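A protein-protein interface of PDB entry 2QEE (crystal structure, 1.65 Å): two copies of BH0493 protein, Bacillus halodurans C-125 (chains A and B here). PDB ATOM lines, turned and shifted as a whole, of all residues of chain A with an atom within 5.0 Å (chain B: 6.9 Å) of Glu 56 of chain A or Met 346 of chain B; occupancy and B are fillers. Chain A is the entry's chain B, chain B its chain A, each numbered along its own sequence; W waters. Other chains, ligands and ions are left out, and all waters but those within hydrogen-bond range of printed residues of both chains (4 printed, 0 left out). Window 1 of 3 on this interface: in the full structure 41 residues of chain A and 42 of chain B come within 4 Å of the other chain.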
ATOM      1  N   TYR A  52      -2.567 -23.670  19.028  1.00  0.00           N
ATOM      2  CA  TYR A  52      -3.688 -24.554  19.370  1.00  0.00           C
ATOM      3  C   TYR A  52      -4.216 -24.184  20.756  1.00  0.00           C
ATOM      4  O   TYR A  52      -5.430 -24.202  21.008  1.00  0.00           O
ATOM      5  CB  TYR A  52      -3.319 -26.050  19.360  1.00  0.00           C
ATOM      6  CG  TYR A  52      -3.038 -26.715  18.034  1.00  0.00           C
ATOM      7  CD1 TYR A  52      -2.482 -26.015  16.957  1.00  0.00           C
ATOM      8  CD2 TYR A  52      -3.267 -28.103  17.868  1.00  0.00           C
ATOM      9  CE1 TYR A  52      -2.195 -26.664  15.748  1.00  0.00           C
ATOM     10  CE2 TYR A  52      -2.982 -28.762  16.653  1.00  0.00           C
ATOM     11  CZ  TYR A  52      -2.437 -28.053  15.616  1.00  0.00           C
ATOM     12  OH  TYR A  52      -2.160 -28.708  14.439  1.00  0.00           O
ATOM     13  N   LEU A  53      -3.299 -23.874  21.686  1.00  0.00           N
ATOM     14  CA  LEU A  53      -3.704 -23.514  23.054  1.00  0.00           C
ATOM     15  C   LEU A  53      -4.184 -22.097  23.202  1.00  0.00           C
ATOM     16  O   LEU A  53      -4.998 -21.835  24.092  1.00  0.00           O
ATOM     17  CB  LEU A  53      -2.604 -23.828  24.097  1.00  0.00           C
ATOM     18  CG  LEU A  53      -2.264 -25.339  24.138  1.00  0.00           C
ATOM     19  CD1 LEU A  53      -1.174 -25.608  25.102  1.00  0.00           C
ATOM     20  CD2 LEU A  53      -3.498 -26.131  24.547  1.00  0.00           C
ATOM     21  N   VAL A  54      -3.685 -21.190  22.356  1.00  0.00           N
ATOM     22  CA  VAL A  54      -4.260 -19.839  22.329  1.00  0.00           C
ATOM     23  C   VAL A  54      -5.761 -19.887  21.951  1.00  0.00           C
ATOM     24  O   VAL A  54      -6.606 -19.269  22.632  1.00  0.00           O
ATOM     25  CB  VAL A  54      -3.494 -18.910  21.438  1.00  0.00           C
ATOM     26  CG1 VAL A  54      -4.162 -17.509  21.393  1.00  0.00           C
ATOM     27  CG2 VAL A  54      -2.037 -18.827  21.928  1.00  0.00           C
ATOM     28  N   ALA A  55      -6.104 -20.678  20.939  1.00  0.00           N
ATOM     29  CA  ALA A  55      -7.548 -20.783  20.577  1.00  0.00           C
ATOM     30  C   ALA A  55      -8.319 -21.310  21.774  1.00  0.00           C
ATOM     31  O   ALA A  55      -9.402 -20.797  22.117  1.00  0.00           O
ATOM     32  CB  ALA A  55      -7.722 -21.699  19.390  1.00  0.00           C
ATOM     33  N   GLU A  56      -7.777 -22.321  22.439  1.00  0.00           N
ATOM     34  CA  GLU A  56      -8.521 -22.953  23.518  1.00  0.00           C
ATOM     35  C   GLU A  56      -8.691 -22.055  24.738  1.00  0.00           C
ATOM     36  O   GLU A  56      -9.755 -21.999  25.353  1.00  0.00           O
ATOM     37  CB  GLU A  56      -7.871 -24.289  23.915  1.00  0.00           C
ATOM     38  CG  GLU A  56      -8.166 -25.402  22.857  1.00  0.00           C
ATOM     39  CD  GLU A  56      -7.510 -26.738  23.146  1.00  0.00           C
ATOM     40  OE1 GLU A  56      -7.504 -27.172  24.311  1.00  0.00           O
ATOM     41  OE2 GLU A  56      -7.028 -27.373  22.171  1.00  0.00           O
ATOM     42  N   VAL A  57      -7.635 -21.319  25.073  1.00  0.00           N
ATOM     43  CA  VAL A  57      -7.742 -20.474  26.253  1.00  0.00           C
ATOM     44  C   VAL A  57      -8.761 -19.363  26.031  1.00  0.00           C
ATOM     45  O   VAL A  57      -9.426 -18.950  26.959  1.00  0.00           O
ATOM     46  CB  VAL A  57      -6.336 -19.935  26.680  1.00  0.00           C
ATOM     47  CG1 VAL A  57      -5.768 -18.882  25.685  1.00  0.00           C
ATOM     48  CG2 VAL A  57      -6.345 -19.469  28.147  1.00  0.00           C
ATOM     49  N   MET A  58      -8.847 -18.863  24.799  1.00  0.00           N
ATOM     50  CA  MET A  58      -9.725 -17.742  24.499  1.00  0.00           C
ATOM     51  C   MET A  58     -11.195 -18.157  24.613  1.00  0.00           C
ATOM     52  O   MET A  58     -12.065 -17.283  24.714  1.00  0.00           O
ATOM     53  CB  MET A  58      -9.424 -17.107  23.128  1.00  0.00           C
ATOM     54  CG  MET A  58      -8.081 -16.388  22.981  1.00  0.00           C
ATOM     55  SD  MET A  58      -7.814 -15.105  24.310  1.00  0.00           S
ATOM     56  CE  MET A  58      -9.289 -14.232  24.279  1.00  0.00           C
ATOM     57  N   ARG A  59     -11.482 -19.474  24.628  1.00  0.00           N
ATOM     58  CA  ARG A  59     -12.878 -19.912  24.832  1.00  0.00           C
ATOM     59  C   ARG A  59     -13.267 -19.809  26.294  1.00  0.00           C
ATOM     60  O   ARG A  59     -14.464 -19.854  26.638  1.00  0.00           O
ATOM     61  CB  ARG A  59     -13.116 -21.363  24.373  1.00  0.00           C
ATOM     62  CG  ARG A  59     -13.229 -21.507  22.856  1.00  0.00           C
ATOM     63  CD  ARG A  59     -13.728 -22.926  22.461  1.00  0.00           C
ATOM     64  NE  ARG A  59     -15.067 -23.144  23.011  1.00  0.00           N
ATOM     65  CZ  ARG A  59     -16.171 -22.490  22.592  1.00  0.00           C
ATOM     66  NH1 ARG A  59     -16.134 -21.654  21.561  1.00  0.00           N
ATOM     67  NH2 ARG A  59     -17.320 -22.737  23.190  1.00  0.00           N
ATOM     68  N   TRP A  60     -12.267 -19.673  27.171  1.00  0.00           N
ATOM     69  CA  TRP A  60     -12.521 -19.630  28.622  1.00  0.00           C
ATOM     70  C   TRP A  60     -12.207 -18.307  29.333  1.00  0.00           C
ATOM     71  O   TRP A  60     -12.941 -17.912  30.238  1.00  0.00           O
ATOM     72  CB  TRP A  60     -11.723 -20.690  29.351  1.00  0.00           C
ATOM     73  CG  TRP A  60     -12.233 -22.116  29.286  1.00  0.00           C
ATOM     74  CD1 TRP A  60     -11.598 -23.194  28.673  1.00  0.00           C
ATOM     75  CD2 TRP A  60     -13.440 -22.628  29.838  1.00  0.00           C
ATOM     76  NE1 TRP A  60     -12.326 -24.322  28.865  1.00  0.00           N
ATOM     77  CE2 TRP A  60     -13.455 -24.036  29.584  1.00  0.00           C
ATOM     78  CE3 TRP A  60     -14.496 -22.060  30.558  1.00  0.00           C
ATOM     79  CZ2 TRP A  60     -14.520 -24.859  29.977  1.00  0.00           C
ATOM     80  CZ3 TRP A  60     -15.557 -22.906  30.992  1.00  0.00           C
ATOM     81  CH2 TRP A  60     -15.559 -24.271  30.678  1.00  0.00           C
ATOM     82  N   LEU A  84      -6.514 -23.631  31.473  1.00  0.00           N
ATOM     83  CA  LEU A  84      -6.728 -24.930  30.798  1.00  0.00           C
ATOM     84  C   LEU A  84      -6.333 -26.198  31.571  1.00  0.00           C
ATOM     85  O   LEU A  84      -6.779 -27.317  31.241  1.00  0.00           O
ATOM     86  CB  LEU A  84      -6.047 -24.880  29.426  1.00  0.00           C
ATOM     87  CG  LEU A  84      -6.474 -23.842  28.387  1.00  0.00           C
ATOM     88  CD1 LEU A  84      -5.851 -24.225  27.043  1.00  0.00           C
ATOM     89  CD2 LEU A  84      -8.015 -23.788  28.310  1.00  0.00           C
ATOM     90  N   SER A  92      -8.199 -31.933  26.689  1.00  0.00           N
ATOM     91  CA  SER A  92      -8.131 -31.766  25.220  1.00  0.00           C
ATOM     92  C   SER A  92      -6.880 -32.423  24.651  1.00  0.00           C
ATOM     93  O   SER A  92      -5.904 -32.638  25.406  1.00  0.00           O
ATOM     94  CB  SER A  92      -8.178 -30.286  24.842  1.00  0.00           C
ATOM     95  OG  SER A  92      -6.917 -29.668  25.001  1.00  0.00           O
ATOM     96  N   ALA A  94      -4.561 -31.173  22.733  1.00  0.00           N
ATOM     97  CA  ALA A  94      -3.391 -30.260  22.768  1.00  0.00           C
ATOM     98  C   ALA A  94      -2.913 -30.154  24.223  1.00  0.00           C
ATOM     99  O   ALA A  94      -1.711 -30.180  24.461  1.00  0.00           O
ATOM    100  CB  ALA A  94      -3.756 -28.860  22.212  1.00  0.00           C
ATOM    101  N   CYS A  95      -3.824 -30.054  25.187  1.00  0.00           N
ATOM    102  CA  CYS A  95      -3.430 -30.033  26.595  1.00  0.00           C
ATOM    103  C   CYS A  95      -2.804 -31.330  27.063  1.00  0.00           C
ATOM    104  O   CYS A  95      -1.707 -31.331  27.686  1.00  0.00           O
ATOM    105  CB  CYS A  95      -4.612 -29.635  27.487  1.00  0.00           C
ATOM    106  SG  CYS A  95      -5.108 -27.913  27.211  1.00  0.00           S
ATOM    107  N   PHE A 329      -6.566 -29.979  12.358  1.00  0.00           N
ATOM    108  CA  PHE A 329      -7.905 -30.329  12.877  1.00  0.00           C
ATOM    109  C   PHE A 329      -8.220 -31.832  12.718  1.00  0.00           C
ATOM    110  O   PHE A 329      -9.172 -32.326  13.290  1.00  0.00           O
ATOM    111  CB  PHE A 329      -8.988 -29.461  12.202  1.00  0.00           C
ATOM    112  CG  PHE A 329      -8.705 -27.987  12.342  1.00  0.00           C
ATOM    113  CD1 PHE A 329      -8.437 -27.467  13.601  1.00  0.00           C
ATOM    114  CD2 PHE A 329      -8.670 -27.158  11.229  1.00  0.00           C
ATOM    115  CE1 PHE A 329      -8.146 -26.078  13.758  1.00  0.00           C
ATOM    116  CE2 PHE A 329      -8.376 -25.785  11.358  1.00  0.00           C
ATOM    117  CZ  PHE A 329      -8.122 -25.253  12.637  1.00  0.00           C
ATOM    118  N   ASN A 332      -6.499 -35.512  15.805  1.00  0.00           N
ATOM    119  CA  ASN A 332      -7.132 -35.779  17.058  1.00  0.00           C
ATOM    120  C   ASN A 332      -7.461 -37.278  17.064  1.00  0.00           C
ATOM    121  O   ASN A 332      -7.837 -37.780  15.987  1.00  0.00           O
ATOM    122  CB  ASN A 332      -8.437 -34.955  17.089  1.00  0.00           C
ATOM    123  CG  ASN A 332      -8.165 -33.458  17.241  1.00  0.00           C
ATOM    124  OD1 ASN A 332      -7.772 -33.026  18.309  1.00  0.00           O
ATOM    125  ND2 ASN A 332      -8.378 -32.672  16.184  1.00  0.00           N
ATOM    126  N   GLN B 308     -20.566 -31.564  11.531  1.00  0.00           N
ATOM    127  CA  GLN B 308     -20.198 -31.577  12.949  1.00  0.00           C
ATOM    128  C   GLN B 308     -18.732 -31.241  13.188  1.00  0.00           C
ATOM    129  O   GLN B 308     -18.413 -30.431  14.074  1.00  0.00           O
ATOM    130  CB  GLN B 308     -20.523 -32.936  13.580  1.00  0.00           C
ATOM    131  CG  GLN B 308     -22.012 -33.303  13.449  1.00  0.00           C
ATOM    132  CD  GLN B 308     -22.912 -32.165  14.054  1.00  0.00           C
ATOM    133  OE1 GLN B 308     -22.540 -31.438  14.996  1.00  0.00           O
ATOM    134  NE2 GLN B 308     -24.077 -32.009  13.474  1.00  0.00           N
ATOM    135  N   HIS B 309     -17.837 -31.842  12.401  1.00  0.00           N
ATOM    136  CA  HIS B 309     -16.426 -31.567  12.692  1.00  0.00           C
ATOM    137  C   HIS B 309     -16.099 -30.105  12.467  1.00  0.00           C
ATOM    138  O   HIS B 309     -15.476 -29.463  13.321  1.00  0.00           O
ATOM    139  CB  HIS B 309     -15.528 -32.469  11.858  1.00  0.00           C
ATOM    140  CG  HIS B 309     -14.074 -32.152  11.995  1.00  0.00           C
ATOM    141  ND1 HIS B 309     -13.462 -31.198  11.216  1.00  0.00           N
ATOM    142  CD2 HIS B 309     -13.125 -32.616  12.845  1.00  0.00           C
ATOM    143  CE1 HIS B 309     -12.185 -31.111  11.559  1.00  0.00           C
ATOM    144  NE2 HIS B 309     -11.958 -31.949  12.554  1.00  0.00           N
ATOM    145  N   GLU B 310     -16.488 -29.562  11.289  1.00  0.00           N
ATOM    146  CA  GLU B 310     -16.239 -28.121  11.044  1.00  0.00           C
ATOM    147  C   GLU B 310     -16.942 -27.176  12.035  1.00  0.00           C
ATOM    148  O   GLU B 310     -16.397 -26.143  12.377  1.00  0.00           O
ATOM    149  CB  GLU B 310     -16.496 -27.790   9.589  1.00  0.00           C
ATOM    150  CG  GLU B 310     -17.939 -27.958   9.185  1.00  0.00           C
ATOM    151  CD  GLU B 310     -18.128 -27.888   7.672  1.00  0.00           C
ATOM    152  OE1 GLU B 310     -17.148 -27.847   6.880  1.00  0.00           O
ATOM    153  OE2 GLU B 310     -19.292 -27.883   7.258  1.00  0.00           O
ATOM    154  N   VAL B 312     -17.150 -27.877  15.228  1.00  0.00           N
ATOM    155  CA  VAL B 312     -16.209 -27.882  16.352  1.00  0.00           C
ATOM    156  C   VAL B 312     -15.026 -26.941  16.043  1.00  0.00           C
ATOM    157  O   VAL B 312     -14.593 -26.177  16.935  1.00  0.00           O
ATOM    158  CB  VAL B 312     -15.654 -29.296  16.603  1.00  0.00           C
ATOM    159  CG1 VAL B 312     -14.612 -29.264  17.760  1.00  0.00           C
ATOM    160  CG2 VAL B 312     -16.827 -30.243  16.998  1.00  0.00           C
ATOM    161  N   VAL B 313     -14.498 -26.994  14.805  1.00  0.00           N
ATOM    162  CA  VAL B 313     -13.381 -26.108  14.455  1.00  0.00           C
ATOM    163  C   VAL B 313     -13.802 -24.647  14.571  1.00  0.00           C
ATOM    164  O   VAL B 313     -13.032 -23.805  15.022  1.00  0.00           O
ATOM    165  CB  VAL B 313     -12.818 -26.445  13.080  1.00  0.00           C
ATOM    166  CG1 VAL B 313     -11.633 -25.473  12.747  1.00  0.00           C
ATOM    167  CG2 VAL B 313     -12.346 -27.919  13.078  1.00  0.00           C
ATOM    168  N   ALA B 315     -15.942 -23.385  16.541  1.00  0.00           N
ATOM    169  CA  ALA B 315     -15.932 -23.090  18.025  1.00  0.00           C
ATOM    170  C   ALA B 315     -14.501 -22.777  18.500  1.00  0.00           C
ATOM    171  O   ALA B 315     -14.306 -21.936  19.391  1.00  0.00           O
ATOM    172  CB  ALA B 315     -16.464 -24.238  18.837  1.00  0.00           C
ATOM    173  N   ARG B 316     -13.504 -23.484  17.965  1.00  0.00           N
ATOM    174  CA  ARG B 316     -12.114 -23.134  18.289  1.00  0.00           C
ATOM    175  C   ARG B 316     -11.796 -21.685  17.918  1.00  0.00           C
ATOM    176  O   ARG B 316     -10.947 -21.065  18.589  1.00  0.00           O
ATOM    177  CB  ARG B 316     -11.130 -24.043  17.572  1.00  0.00           C
ATOM    178  CG  ARG B 316     -11.154 -25.483  18.065  1.00  0.00           C
ATOM    179  CD  ARG B 316     -10.015 -26.307  17.390  1.00  0.00           C
ATOM    180  NE  ARG B 316      -8.698 -25.687  17.621  1.00  0.00           N
ATOM    181  CZ  ARG B 316      -7.919 -25.907  18.676  1.00  0.00           C
ATOM    182  NH1 ARG B 316      -8.317 -26.695  19.695  1.00  0.00           N
ATOM    183  NH2 ARG B 316      -6.735 -25.276  18.737  1.00  0.00           N
ATOM    184  N   ARG B 341     -16.535 -37.079  21.184  1.00  0.00           N
ATOM    185  CA  ARG B 341     -15.064 -37.250  21.169  1.00  0.00           C
ATOM    186  C   ARG B 341     -14.384 -36.133  20.389  1.00  0.00           C
ATOM    187  O   ARG B 341     -13.366 -35.608  20.869  1.00  0.00           O
ATOM    188  CB  ARG B 341     -14.650 -38.622  20.595  1.00  0.00           C
ATOM    189  CG  ARG B 341     -15.118 -39.724  21.592  1.00  0.00           C
ATOM    190  CD  ARG B 341     -14.904 -41.144  21.091  1.00  0.00           C
ATOM    191  NE  ARG B 341     -15.264 -42.068  22.155  1.00  0.00           N
ATOM    192  CZ  ARG B 341     -14.423 -42.453  23.139  1.00  0.00           C
ATOM    193  NH1 ARG B 341     -13.140 -42.068  23.143  1.00  0.00           N
ATOM    194  NH2 ARG B 341     -14.874 -43.270  24.089  1.00  0.00           N
ATOM    195  N   MET B 342     -14.919 -35.767  19.218  1.00  0.00           N
ATOM    196  CA  MET B 342     -14.325 -34.700  18.378  1.00  0.00           C
ATOM    197  C   MET B 342     -14.390 -33.390  19.222  1.00  0.00           C
ATOM    198  O   MET B 342     -13.427 -32.617  19.281  1.00  0.00           O
ATOM    199  CB  MET B 342     -15.074 -34.489  17.034  1.00  0.00           C
ATOM    200  CG  MET B 342     -14.889 -35.671  16.074  1.00  0.00           C
ATOM    201  SD  MET B 342     -15.537 -35.245  14.438  1.00  0.00           S
ATOM    202  CE  MET B 342     -17.309 -35.145  14.845  1.00  0.00           C
ATOM    203  N   ARG B 343     -15.532 -33.187  19.894  1.00  0.00           N
ATOM    204  CA  ARG B 343     -15.739 -31.969  20.642  1.00  0.00           C
ATOM    205  C   ARG B 343     -14.735 -31.870  21.817  1.00  0.00           C
ATOM    206  O   ARG B 343     -14.079 -30.837  21.956  1.00  0.00           O
ATOM    207  CB  ARG B 343     -17.202 -31.905  21.143  1.00  0.00           C
ATOM    208  CG  ARG B 343     -18.164 -31.472  20.052  1.00  0.00           C
ATOM    209  CD  ARG B 343     -19.572 -31.841  20.513  1.00  0.00           C
ATOM    210  NE  ARG B 343     -20.492 -31.231  19.523  1.00  0.00           N
ATOM    211  CZ  ARG B 343     -21.792 -31.106  19.760  1.00  0.00           C
ATOM    212  NH1 ARG B 343     -22.291 -31.620  20.865  1.00  0.00           N
ATOM    213  NH2 ARG B 343     -22.576 -30.475  18.902  1.00  0.00           N
ATOM    214  N   MET B 344     -14.608 -32.923  22.608  1.00  0.00           N
ATOM    215  CA  MET B 344     -13.717 -32.900  23.729  1.00  0.00           C
ATOM    216  C   MET B 344     -12.262 -32.821  23.277  1.00  0.00           C
ATOM    217  O   MET B 344     -11.440 -32.145  23.925  1.00  0.00           O
ATOM    218  CB  MET B 344     -13.937 -34.109  24.584  1.00  0.00           C
ATOM    219  CG  MET B 344     -13.190 -33.974  25.965  1.00  0.00           C
ATOM    220  SD  MET B 344     -13.792 -35.127  27.226  1.00  0.00           S
ATOM    221  CE  MET B 344     -15.440 -34.438  27.547  1.00  0.00           C
ATOM    222  N   GLU B 345     -11.917 -33.493  22.173  1.00  0.00           N
ATOM    223  CA  GLU B 345     -10.521 -33.460  21.713  1.00  0.00           C
ATOM    224  C   GLU B 345     -10.059 -32.039  21.294  1.00  0.00           C
ATOM    225  O   GLU B 345      -8.918 -31.654  21.567  1.00  0.00           O
ATOM    226  CB  GLU B 345     -10.235 -34.476  20.558  1.00  0.00           C
ATOM    227  CG  GLU B 345     -10.318 -35.847  21.159  1.00  0.00           C
ATOM    228  CD  GLU B 345     -10.435 -37.060  20.207  1.00  0.00           C
ATOM    229  OE1 GLU B 345     -10.369 -36.889  18.966  1.00  0.00           O
ATOM    230  OE2 GLU B 345     -10.568 -38.198  20.770  1.00  0.00           O
ATOM    231  N   MET B 346     -10.973 -31.240  20.744  1.00  0.00           N
ATOM    232  CA  MET B 346     -10.629 -29.918  20.197  1.00  0.00           C
ATOM    233  C   MET B 346     -11.101 -28.786  21.094  1.00  0.00           C
ATOM    234  O   MET B 346     -10.668 -27.661  20.892  1.00  0.00           O
ATOM    235  CB  MET B 346     -11.238 -29.705  18.818  1.00  0.00           C
ATOM    236  CG  MET B 346     -10.334 -30.232  17.719  1.00  0.00           C
ATOM    237  SD  MET B 346     -11.034 -30.007  16.060  1.00  0.00           S
ATOM    238  CE  MET B 346     -12.178 -31.401  16.069  1.00  0.00           C
ATOM    239  N   LEU B 347     -11.965 -29.071  22.051  1.00  0.00           N
ATOM    240  CA  LEU B 347     -12.507 -27.975  22.917  1.00  0.00           C
ATOM    241  C   LEU B 347     -12.346 -28.255  24.409  1.00  0.00           C
ATOM    242  O   LEU B 347     -12.805 -27.464  25.234  1.00  0.00           O
ATOM    243  CB  LEU B 347     -13.992 -27.707  22.615  1.00  0.00           C
ATOM    244  CG  LEU B 347     -14.378 -27.413  21.158  1.00  0.00           C
ATOM    245  CD1 LEU B 347     -15.910 -27.293  21.090  1.00  0.00           C
ATOM    246  CD2 LEU B 347     -13.703 -26.167  20.604  1.00  0.00           C
ATOM    247  N   GLY B 348     -11.736 -29.379  24.785  1.00  0.00           N
ATOM    248  CA  GLY B 348     -11.665 -29.726  26.205  1.00  0.00           C
ATOM    249  C   GLY B 348     -13.095 -29.765  26.792  1.00  0.00           C
ATOM    250  O   GLY B 348     -13.944 -30.522  26.337  1.00  0.00           O
ATOM    251  N   SER B 350     -15.083 -27.075  27.046  1.00  0.00           N
ATOM    252  CA  SER B 350     -15.746 -25.801  26.679  1.00  0.00           C
ATOM    253  C   SER B 350     -16.920 -25.963  25.683  1.00  0.00           C
ATOM    254  O   SER B 350     -17.057 -25.197  24.725  1.00  0.00           O
ATOM    255  CB  SER B 350     -14.719 -24.716  26.212  1.00  0.00           C
ATOM    256  OG  SER B 350     -14.080 -25.058  24.982  1.00  0.00           O
HETATM  257  O   HOH W   1      -9.681 -26.680  25.860  1.00  0.00           O
HETATM  258  O   HOH W   2     -11.222 -24.407  24.996  1.00  0.00           O
HETATM  259  O   HOH W   3     -11.065 -19.098  20.641  1.00  0.00           O
HETATM  260  O   HOH W   4      -6.816 -29.928  21.443  1.00  0.00           O
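O of Phe 329 of chain A sits at hydrogen-bond distance from NE2 of His 309 of chain B. O of Ala 315 of chain B is in hydrogen-bond range of NH1 of Arg 59 of chain A. The backbone carbonyl oxygen (O) of Tyr 52 of chain A lies within hydrogen-bond range of the guanidinium group (NH2) of Arg 316 of chain B (2.8 Å). The side-chain carboxylate (OE2) of Glu 56 of chain A lies within salt-bridge range of the guanidinium group (NH1) of Arg 316 of chain B. The side-chain sulfur (SD) of Met 346 of chain B sits close to the side-chain amide nitrogen (ND2) of Asn 332 of chain A, 3.8 Å away. The backbone carbonyl oxygen (O) of Ser 350 of chain B sits at hydrogen-bond distance from the guanidinium group (NH2) of Arg 59 of chain A.
O of Met 346 of chain B sits at hydrogen-bond distance from NH1 of Arg 316 of chain B, at 2.8 Å. The backbone carbonyl oxygen of Leu 347 of chain B is in hydrogen-bond range of the side-chain hydroxyl of Ser 350 of chain B, at 2.7 Å. The side-chain hydroxyl of Ser 92 of chain A lies within hydrogen-bond range of the side-chain carboxylate of Glu 56 of chain A, 2.7 Å away. The side-chain hydroxyl (OG) of Ser 92 of chain A lies within hydrogen-bond range of the backbone NH (N) of Cys 95 of chain A (3.1 Å). The side-chain amide nitrogen (ND2) of Asn 332 of chain A lies within hydrogen-bond range of the backbone carbonyl oxygen (O) of Phe 329 of chain A (3.0 Å).
Among the printed residues, pairs that only touch across the chains: Asn 332 of chain A with Glu 345 of chain B, Ala 55 of chain A with Arg 316 of chain B, Phe 329 of chain A with Val 313 of chain B, Ser 92 of chain A with Met 344 of chain B, Trp 60 of chain A with Ser 350 of chain B, Ser 92 of chain A with Glu 345 of chain B, Ser 92 of chain A with Gly 348 of chain B, Arg 59 of chain A with Leu 347 of chain B, Glu 56 of chain A with Met 346 of chain B and Phe 329 of chain A with Arg 316 of chain B.
Met 346 of chain B touches just these residues of chain A: Glu 56 (3.9 Å) and Asn 332 (3.5 Å). Of the printed residues of chain B, Trp 60 of chain A touches Ser 350. Of the printed residues of chain B, Ser 92 of chain A touches Met 344, Glu 345 and Gly 348. Of the printed residues of chain A, Ser 350 of chain B touches Arg 59 (2.9 Å) and Trp 60 (3.6 Å). The nearest residue of chain B that does not touch Glu 56 of chain A is Glu 345 of chain B (4.7 Å). The nearest residue of chain A that does not touch Met 346 of chain B is Phe 329 of chain A (4.1 Å).
Of the 16 printed residues of chain B, 10 touch a printed residue of chain A. Hydrophobic or aromatic side chains of chain B that line the printed part of chain A: His 309, Val 313, Ala 315, Met 346 and Leu 347. Of the 15 printed residues of chain A, 8 touch a printed residue of chain B. Among the printed residues, Asp or Glu carboxylates within 4 Å of a Lys or Arg side-chain nitrogen of the other chain: Glu 56 of chain A with Arg 316 of chain B (2.9 Å).
No position is printed for both chains.
Water W4 lies within hydrogen-bond range of the side-chain carboxylate of Glu 56 of chain A (2.7 Å), the backbone carbonyl oxygen of Glu 345 of chain B (2.7 Å) and the backbone NH of Ala 94 of chain A (2.9 Å). Water W1 bridges the side-chain carboxylate (OE1) of Glu 56 of chain A (2.7 Å) and the backbone carbonyl oxygen (O) of Leu 347 of chain B (3.3 Å). Water W3 lies within hydrogen-bond range of the backbone carbonyl oxygen of Ala 55 of chain A and the backbone carbonyl oxygen of Arg 316 of chain B. Water W2 lies within hydrogen-bond range of O of Glu 56 of chain A (2.8 Å), OG of Ser 350 of chain B (2.9 Å) and O of Leu 347 of chain B (3.5 Å).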
